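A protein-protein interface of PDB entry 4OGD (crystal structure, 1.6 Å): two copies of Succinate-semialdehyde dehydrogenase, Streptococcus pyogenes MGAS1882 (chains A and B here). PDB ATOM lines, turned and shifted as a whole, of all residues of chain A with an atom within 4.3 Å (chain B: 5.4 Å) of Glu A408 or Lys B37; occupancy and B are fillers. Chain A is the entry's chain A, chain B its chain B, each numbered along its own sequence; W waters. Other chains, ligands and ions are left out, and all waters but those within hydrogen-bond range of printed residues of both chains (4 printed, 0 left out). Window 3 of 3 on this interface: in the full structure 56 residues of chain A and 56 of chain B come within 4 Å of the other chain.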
ATOM      1  N   ASN A 382      14.423 -13.298 -10.096  1.00  0.00           N
ATOM      2  CA  ASN A 382      14.648 -14.178  -8.950  1.00  0.00           C
ATOM      3  C   ASN A 382      15.550 -15.360  -9.259  1.00  0.00           C
ATOM      4  O   ASN A 382      15.978 -16.065  -8.339  1.00  0.00           O
ATOM      5  CB  ASN A 382      13.318 -14.670  -8.374  1.00  0.00           C
ATOM      6  CG  ASN A 382      12.538 -13.562  -7.712  1.00  0.00           C
ATOM      7  OD1 ASN A 382      13.107 -12.533  -7.356  1.00  0.00           O
ATOM      8  ND2 ASN A 382      11.232 -13.765  -7.528  1.00  0.00           N
ATOM      9  N   GLY A 387      20.708 -11.370  -4.142  1.00  0.00           N
ATOM     10  CA  GLY A 387      19.429 -10.761  -3.838  1.00  0.00           C
ATOM     11  C   GLY A 387      19.653  -9.574  -2.931  1.00  0.00           C
ATOM     12  O   GLY A 387      19.226  -9.580  -1.780  1.00  0.00           O
ATOM     13  N   LYS A 406       7.254  -9.296  -4.804  1.00  0.00           N
ATOM     14  CA  LYS A 406       7.488 -10.605  -5.410  1.00  0.00           C
ATOM     15  C   LYS A 406       8.958 -10.896  -5.711  1.00  0.00           C
ATOM     16  O   LYS A 406       9.309 -12.031  -6.043  1.00  0.00           O
ATOM     17  CB  LYS A 406       6.647 -10.767  -6.677  1.00  0.00           C
ATOM     18  CG  LYS A 406       5.158 -10.781  -6.390  1.00  0.00           C
ATOM     19  CD  LYS A 406       4.350 -10.871  -7.678  1.00  0.00           C
ATOM     20  CE  LYS A 406       2.863 -10.965  -7.371  1.00  0.00           C
ATOM     21  NZ  LYS A 406       2.066 -10.915  -8.628  1.00  0.00           N
ATOM     22  N   ILE A 407       9.814  -9.887  -5.593  1.00  0.00           N
ATOM     23  CA  ILE A 407      11.239 -10.085  -5.859  1.00  0.00           C
ATOM     24  C   ILE A 407      11.951 -10.615  -4.620  1.00  0.00           C
ATOM     25  O   ILE A 407      11.777 -10.084  -3.512  1.00  0.00           O
ATOM     26  CB  ILE A 407      11.939  -8.785  -6.324  1.00  0.00           C
ATOM     27  CG1 ILE A 407      11.155  -8.124  -7.464  1.00  0.00           C
ATOM     28  CG2 ILE A 407      13.360  -9.086  -6.788  1.00  0.00           C
ATOM     29  CD1 ILE A 407      10.887  -9.061  -8.644  1.00  0.00           C
ATOM     30  N   GLU A 408      12.743 -11.668  -4.812  1.00  0.00           N
ATOM     31  CA  GLU A 408      13.548 -12.255  -3.748  1.00  0.00           C
ATOM     32  C   GLU A 408      14.833 -11.445  -3.601  1.00  0.00           C
ATOM     33  O   GLU A 408      15.857 -11.739  -4.236  1.00  0.00           O
ATOM     34  CB  GLU A 408      13.861 -13.720  -4.075  1.00  0.00           C
ATOM     35  CG  GLU A 408      12.622 -14.598  -4.062  1.00  0.00           C
ATOM     36  CD  GLU A 408      12.914 -16.046  -4.396  1.00  0.00           C
ATOM     37  OE1 GLU A 408      13.936 -16.321  -5.058  1.00  0.00           O
ATOM     38  OE2 GLU A 408      12.104 -16.911  -4.001  1.00  0.00           O
ATOM     39  N   THR A 409      14.763 -10.408  -2.773  1.00  0.00           N
ATOM     40  CA  THR A 409      15.868  -9.478  -2.601  1.00  0.00           C
ATOM     41  C   THR A 409      15.642  -8.663  -1.336  1.00  0.00           C
ATOM     42  O   THR A 409      14.518  -8.579  -0.838  1.00  0.00           O
ATOM     43  CB  THR A 409      15.981  -8.524  -3.811  1.00  0.00           C
ATOM     44  OG1 THR A 409      17.221  -7.820  -3.740  1.00  0.00           O
ATOM     45  CG2 THR A 409      14.834  -7.519  -3.825  1.00  0.00           C
ATOM     46  N   ILE A 429      19.877 -11.110   0.740  1.00  0.00           N
ATOM     47  CA  ILE A 429      19.656 -12.525   1.014  1.00  0.00           C
ATOM     48  C   ILE A 429      20.505 -13.314   0.019  1.00  0.00           C
ATOM     49  O   ILE A 429      21.245 -12.722  -0.773  1.00  0.00           O
ATOM     50  CB  ILE A 429      18.169 -12.916   0.858  1.00  0.00           C
ATOM     51  CG1 ILE A 429      17.695 -12.615  -0.563  1.00  0.00           C
ATOM     52  CG2 ILE A 429      17.317 -12.171   1.887  1.00  0.00           C
ATOM     53  CD1 ILE A 429      16.256 -13.084  -0.866  1.00  0.00           C
ATOM     54  N   LYS A 430      20.400 -14.641   0.061  1.00  0.00           N
ATOM     55  CA  LYS A 430      21.186 -15.516  -0.819  1.00  0.00           C
ATOM     56  C   LYS A 430      22.683 -15.194  -0.709  1.00  0.00           C
ATOM     57  O   LYS A 430      23.184 -14.988   0.407  1.00  0.00           O
ATOM     58  CB  LYS A 430      20.665 -15.469  -2.270  1.00  0.00           C
ATOM     59  CG  LYS A 430      19.186 -15.878  -2.380  1.00  0.00           C
ATOM     60  CD  LYS A 430      18.683 -15.868  -3.832  1.00  0.00           C
ATOM     61  CE  LYS A 430      17.167 -16.107  -3.909  1.00  0.00           C
ATOM     62  NZ  LYS A 430      16.675 -16.060  -5.341  1.00  0.00           N
ATOM     63  N   ALA B  32      10.494 -29.465   0.047  1.00  0.00           N
ATOM     64  CA  ALA B  32      10.549 -28.309   0.941  1.00  0.00           C
ATOM     65  C   ALA B  32      10.693 -27.006   0.160  1.00  0.00           C
ATOM     66  O   ALA B  32      10.046 -26.005   0.480  1.00  0.00           O
ATOM     67  CB  ALA B  32      11.693 -28.468   1.947  1.00  0.00           C
ATOM     68  N   HIS B  33      11.551 -27.011  -0.857  1.00  0.00           N
ATOM     69  CA  HIS B  33      11.738 -25.823  -1.684  1.00  0.00           C
ATOM     70  C   HIS B  33      10.455 -25.439  -2.413  1.00  0.00           C
ATOM     71  O   HIS B  33      10.118 -24.255  -2.501  1.00  0.00           O
ATOM     72  CB  HIS B  33      12.848 -26.047  -2.709  1.00  0.00           C
ATOM     73  CG  HIS B  33      13.033 -24.904  -3.657  1.00  0.00           C
ATOM     74  ND1 HIS B  33      13.458 -23.658  -3.248  1.00  0.00           N
ATOM     75  CD2 HIS B  33      12.849 -24.818  -4.996  1.00  0.00           C
ATOM     76  CE1 HIS B  33      13.531 -22.853  -4.296  1.00  0.00           C
ATOM     77  NE2 HIS B  33      13.164 -23.532  -5.370  1.00  0.00           N
ATOM     78  N   LEU B  34       9.735 -26.435  -2.919  1.00  0.00           N
ATOM     79  CA  LEU B  34       8.533 -26.152  -3.691  1.00  0.00           C
ATOM     80  C   LEU B  34       7.442 -25.632  -2.758  1.00  0.00           C
ATOM     81  O   LEU B  34       6.614 -24.824  -3.167  1.00  0.00           O
ATOM     82  CB  LEU B  34       8.072 -27.386  -4.474  1.00  0.00           C
ATOM     83  CG  LEU B  34       9.034 -27.826  -5.581  1.00  0.00           C
ATOM     84  CD1 LEU B  34       8.568 -29.137  -6.207  1.00  0.00           C
ATOM     85  CD2 LEU B  34       9.194 -26.754  -6.635  1.00  0.00           C
ATOM     86  N   LEU B  35       7.477 -26.069  -1.497  1.00  0.00           N
ATOM     87  CA  LEU B  35       6.515 -25.609  -0.505  1.00  0.00           C
ATOM     88  C   LEU B  35       6.788 -24.155  -0.153  1.00  0.00           C
ATOM     89  O   LEU B  35       5.860 -23.356  -0.018  1.00  0.00           O
ATOM     90  CB  LEU B  35       6.560 -26.482   0.753  1.00  0.00           C
ATOM     91  CG  LEU B  35       5.491 -26.219   1.821  1.00  0.00           C
ATOM     92  CD1 LEU B  35       4.087 -26.241   1.181  1.00  0.00           C
ATOM     93  CD2 LEU B  35       5.591 -27.233   2.953  1.00  0.00           C
ATOM     94  N   TYR B  36       8.067 -23.812  -0.015  1.00  0.00           N
ATOM     95  CA  TYR B  36       8.449 -22.416   0.196  1.00  0.00           C
ATOM     96  C   TYR B  36       7.903 -21.550  -0.938  1.00  0.00           C
ATOM     97  O   TYR B  36       7.323 -20.490  -0.701  1.00  0.00           O
ATOM     98  CB  TYR B  36       9.973 -22.267   0.274  1.00  0.00           C
ATOM     99  CG  TYR B  36      10.436 -20.893  -0.153  1.00  0.00           C
ATOM    100  CD1 TYR B  36      10.334 -19.804   0.706  1.00  0.00           C
ATOM    101  CD2 TYR B  36      10.933 -20.676  -1.436  1.00  0.00           C
ATOM    102  CE1 TYR B  36      10.733 -18.534   0.297  1.00  0.00           C
ATOM    103  CE2 TYR B  36      11.328 -19.419  -1.851  1.00  0.00           C
ATOM    104  CZ  TYR B  36      11.228 -18.354  -0.983  1.00  0.00           C
ATOM    105  OH  TYR B  36      11.619 -17.103  -1.418  1.00  0.00           O
ATOM    106  N   LYS B  37       8.097 -22.000  -2.173  1.00  0.00           N
ATOM    107  CA  LYS B  37       7.638 -21.227  -3.325  1.00  0.00           C
ATOM    108  C   LYS B  37       6.116 -21.095  -3.317  1.00  0.00           C
ATOM    109  O   LYS B  37       5.583 -20.021  -3.591  1.00  0.00           O
ATOM    110  CB  LYS B  37       8.126 -21.854  -4.633  1.00  0.00           C
ATOM    111  CG  LYS B  37       9.616 -21.648  -4.913  1.00  0.00           C
ATOM    112  CD  LYS B  37       9.934 -20.187  -5.248  1.00  0.00           C
ATOM    113  CE  LYS B  37      11.371 -20.027  -5.743  1.00  0.00           C
ATOM    114  NZ  LYS B  37      11.695 -18.615  -6.094  1.00  0.00           N
ATOM    115  N   LYS B  38       5.424 -22.173  -2.968  1.00  0.00           N
ATOM    116  CA  LYS B  38       3.965 -22.158  -2.923  1.00  0.00           C
ATOM    117  C   LYS B  38       3.462 -21.116  -1.924  1.00  0.00           C
ATOM    118  O   LYS B  38       2.537 -20.362  -2.212  1.00  0.00           O
ATOM    119  CB  LYS B  38       3.419 -23.543  -2.582  1.00  0.00           C
ATOM    120  CG  LYS B  38       1.909 -23.587  -2.320  1.00  0.00           C
ATOM    121  CD  LYS B  38       1.454 -25.018  -2.041  1.00  0.00           C
ATOM    122  CE  LYS B  38      -0.029 -25.069  -1.696  1.00  0.00           C
ATOM    123  NZ  LYS B  38      -0.530 -26.476  -1.607  1.00  0.00           N
ATOM    124  N   TRP B  39       4.095 -21.069  -0.758  1.00  0.00           N
ATOM    125  CA  TRP B  39       3.682 -20.161   0.305  1.00  0.00           C
ATOM    126  C   TRP B  39       4.065 -18.708   0.022  1.00  0.00           C
ATOM    127  O   TRP B  39       3.460 -17.785   0.570  1.00  0.00           O
ATOM    128  CB  TRP B  39       4.263 -20.630   1.638  1.00  0.00           C
ATOM    129  CG  TRP B  39       3.610 -21.871   2.212  1.00  0.00           C
ATOM    130  CD1 TRP B  39       2.395 -22.415   1.879  1.00  0.00           C
ATOM    131  CD2 TRP B  39       4.150 -22.697   3.247  1.00  0.00           C
ATOM    132  NE1 TRP B  39       2.151 -23.531   2.658  1.00  0.00           N
ATOM    133  CE2 TRP B  39       3.220 -23.727   3.496  1.00  0.00           C
ATOM    134  CE3 TRP B  39       5.336 -22.667   3.982  1.00  0.00           C
ATOM    135  CZ2 TRP B  39       3.441 -24.718   4.460  1.00  0.00           C
ATOM    136  CZ3 TRP B  39       5.556 -23.656   4.941  1.00  0.00           C
ATOM    137  CH2 TRP B  39       4.609 -24.659   5.174  1.00  0.00           C
ATOM    138  N   ARG B  40       5.053 -18.502  -0.845  1.00  0.00           N
ATOM    139  CA  ARG B  40       5.391 -17.171  -1.331  1.00  0.00           C
ATOM    140  C   ARG B  40       4.363 -16.697  -2.339  1.00  0.00           C
ATOM    141  O   ARG B  40       3.939 -15.543  -2.315  1.00  0.00           O
ATOM    142  CB  ARG B  40       6.747 -17.192  -2.026  1.00  0.00           C
ATOM    143  CG  ARG B  40       7.910 -17.194  -1.092  1.00  0.00           C
ATOM    144  CD  ARG B  40       7.968 -15.904  -0.289  1.00  0.00           C
ATOM    145  NE  ARG B  40       8.001 -14.730  -1.143  1.00  0.00           N
ATOM    146  CZ  ARG B  40       9.006 -13.865  -1.193  1.00  0.00           C
ATOM    147  NH1 ARG B  40      10.071 -14.038  -0.429  1.00  0.00           N
ATOM    148  NH2 ARG B  40       8.939 -12.824  -2.014  1.00  0.00           N
ATOM    149  N   LYS B  41       3.977 -17.594  -3.235  1.00  0.00           N
ATOM    150  CA  LYS B  41       3.123 -17.233  -4.369  1.00  0.00           C
ATOM    151  C   LYS B  41       1.623 -17.295  -4.061  1.00  0.00           C
ATOM    152  O   LYS B  41       0.802 -16.794  -4.834  1.00  0.00           O
ATOM    153  CB  LYS B  41       3.448 -18.131  -5.565  1.00  0.00           C
ATOM    154  CG  LYS B  41       4.888 -18.011  -6.074  1.00  0.00           C
ATOM    155  CD  LYS B  41       5.142 -19.066  -7.145  1.00  0.00           C
ATOM    156  CE  LYS B  41       6.599 -19.118  -7.605  1.00  0.00           C
ATOM    157  NZ  LYS B  41       6.840 -18.245  -8.777  1.00  0.00           N
ATOM    158  N   GLU B  42       1.263 -17.919  -2.942  1.00  0.00           N
ATOM    159  CA  GLU B  42      -0.134 -18.048  -2.532  1.00  0.00           C
ATOM    160  C   GLU B  42      -0.192 -17.790  -1.039  1.00  0.00           C
ATOM    161  O   GLU B  42       0.679 -18.245  -0.307  1.00  0.00           O
ATOM    162  CB  GLU B  42      -0.661 -19.465  -2.798  1.00  0.00           C
ATOM    163  CG  GLU B  42      -0.616 -19.937  -4.248  1.00  0.00           C
ATOM    164  CD  GLU B  42      -1.039 -21.388  -4.407  1.00  0.00           C
ATOM    165  OE1 GLU B  42      -1.403 -22.034  -3.401  1.00  0.00           O
ATOM    166  OE2 GLU B  42      -1.013 -21.899  -5.550  1.00  0.00           O
ATOM    167  N   ASN B 448      13.407 -12.307   5.644  1.00  0.00           N
ATOM    168  CA  ASN B 448      13.961 -11.270   4.793  1.00  0.00           C
ATOM    169  C   ASN B 448      13.284  -9.959   5.149  1.00  0.00           C
ATOM    170  O   ASN B 448      12.095  -9.778   4.875  1.00  0.00           O
ATOM    171  CB  ASN B 448      13.697 -11.623   3.326  1.00  0.00           C
ATOM    172  CG  ASN B 448      14.071 -10.503   2.370  1.00  0.00           C
ATOM    173  OD1 ASN B 448      14.706  -9.526   2.752  1.00  0.00           O
ATOM    174  ND2 ASN B 448      13.686 -10.658   1.104  1.00  0.00           N
HETATM  175  O   HOH W   1      14.228 -19.174  -3.888  1.00  0.00           O
HETATM  176  O   HOH W   2      14.097 -18.319  -7.608  1.00  0.00           O
HETATM  177  O   HOH W   3      11.455 -11.418  -1.203  1.00  0.00           O
HETATM  178  O   HOH W   4       9.180 -16.375  -5.241  1.00  0.00           O
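The backbone NH of Glu A408 sits at hydrogen-bond distance from the side-chain amide oxygen of Asn A382.
The backbone carbonyl oxygen of Gly A387 sits close to the side-chain hydroxyl of Thr A409, at 3.3 Å.
The backbone carbonyl oxygen of Gly A387 is in hydrogen-bond range of the backbone NH of Ile A429.
OE1 of Glu A408 is in salt-bridge range of NZ of Lys A430, 2.8 Å away.
Ile A429 touches Asn B448 (CG2 to CG, 3.7 Å).
No position is printed for both chains.
Of the 4 pairs that touch across the chains among the printed residues, none has its exchanged pair printed and touching as well.
Water W3 lies within hydrogen-bond range of the backbone carbonyl oxygen of Ile A407, the guanidinium group of Arg B40 and the side-chain amide nitrogen of Asn B448.
Water W2 lies within hydrogen-bond range of the side-chain amino group (NZ) of Lys B37 (2.9 Å), the backbone carbonyl oxygen (O) of Asn A382 (3.0 Å) and the side-chain carboxylate (OE1) of Glu A408 (3.2 Å).
Water W1 lies within hydrogen-bond range of the side-chain carboxylate (OE1) of Glu A408 and the side-chain amino group (NZ) of Lys B37.
Water W4 lies within hydrogen-bond range of the side-chain carboxylate (OE2) of Glu A408 (3.2 Å) and the side-chain amino group (NZ) of Lys B37 (3.5 Å).
Glu A408 touches just these residues of chain B: Tyr B36 and Lys B37.
Lys B37 touches one residue of chain A.
Of the printed residues of chain A, Tyr B36 touches Glu A408 (2.6 Å).
Of the printed residues of chain B, Ile A429 touches Asn B448.
Printed residues of chain B within 4 Å of Thr A409: Asn B448 (3.0 Å).
Lys A406 touches none of the printed residues of chain B.
The nearest residue of chain B that does not touch Glu A408 is Arg B40 (4.5 Å).
The nearest printed residue of chain A that does not touch Asn B448 is Glu A408 (4.9 Å).
The side-chain hydroxyl of Tyr B36 sits at hydrogen-bond distance from the side-chain carboxylate of Glu A408, at 2.6 Å.
The side-chain amino group (NZ) of Lys B37 lies within salt-bridge range of the side-chain carboxylate (OE2) of Glu A408, 2.7 Å away.
ND2 of Asn B448 lies within hydrogen-bond range of O of Thr A409 (3.0 Å).
Along chain B the printed residues that touch a printed residue of chain A span positions 36 to 448.
Along chain A the printed residues that touch a printed residue of chain B span positions 408 to 429.
Among the printed residues, 4 pairs touch across the chains.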
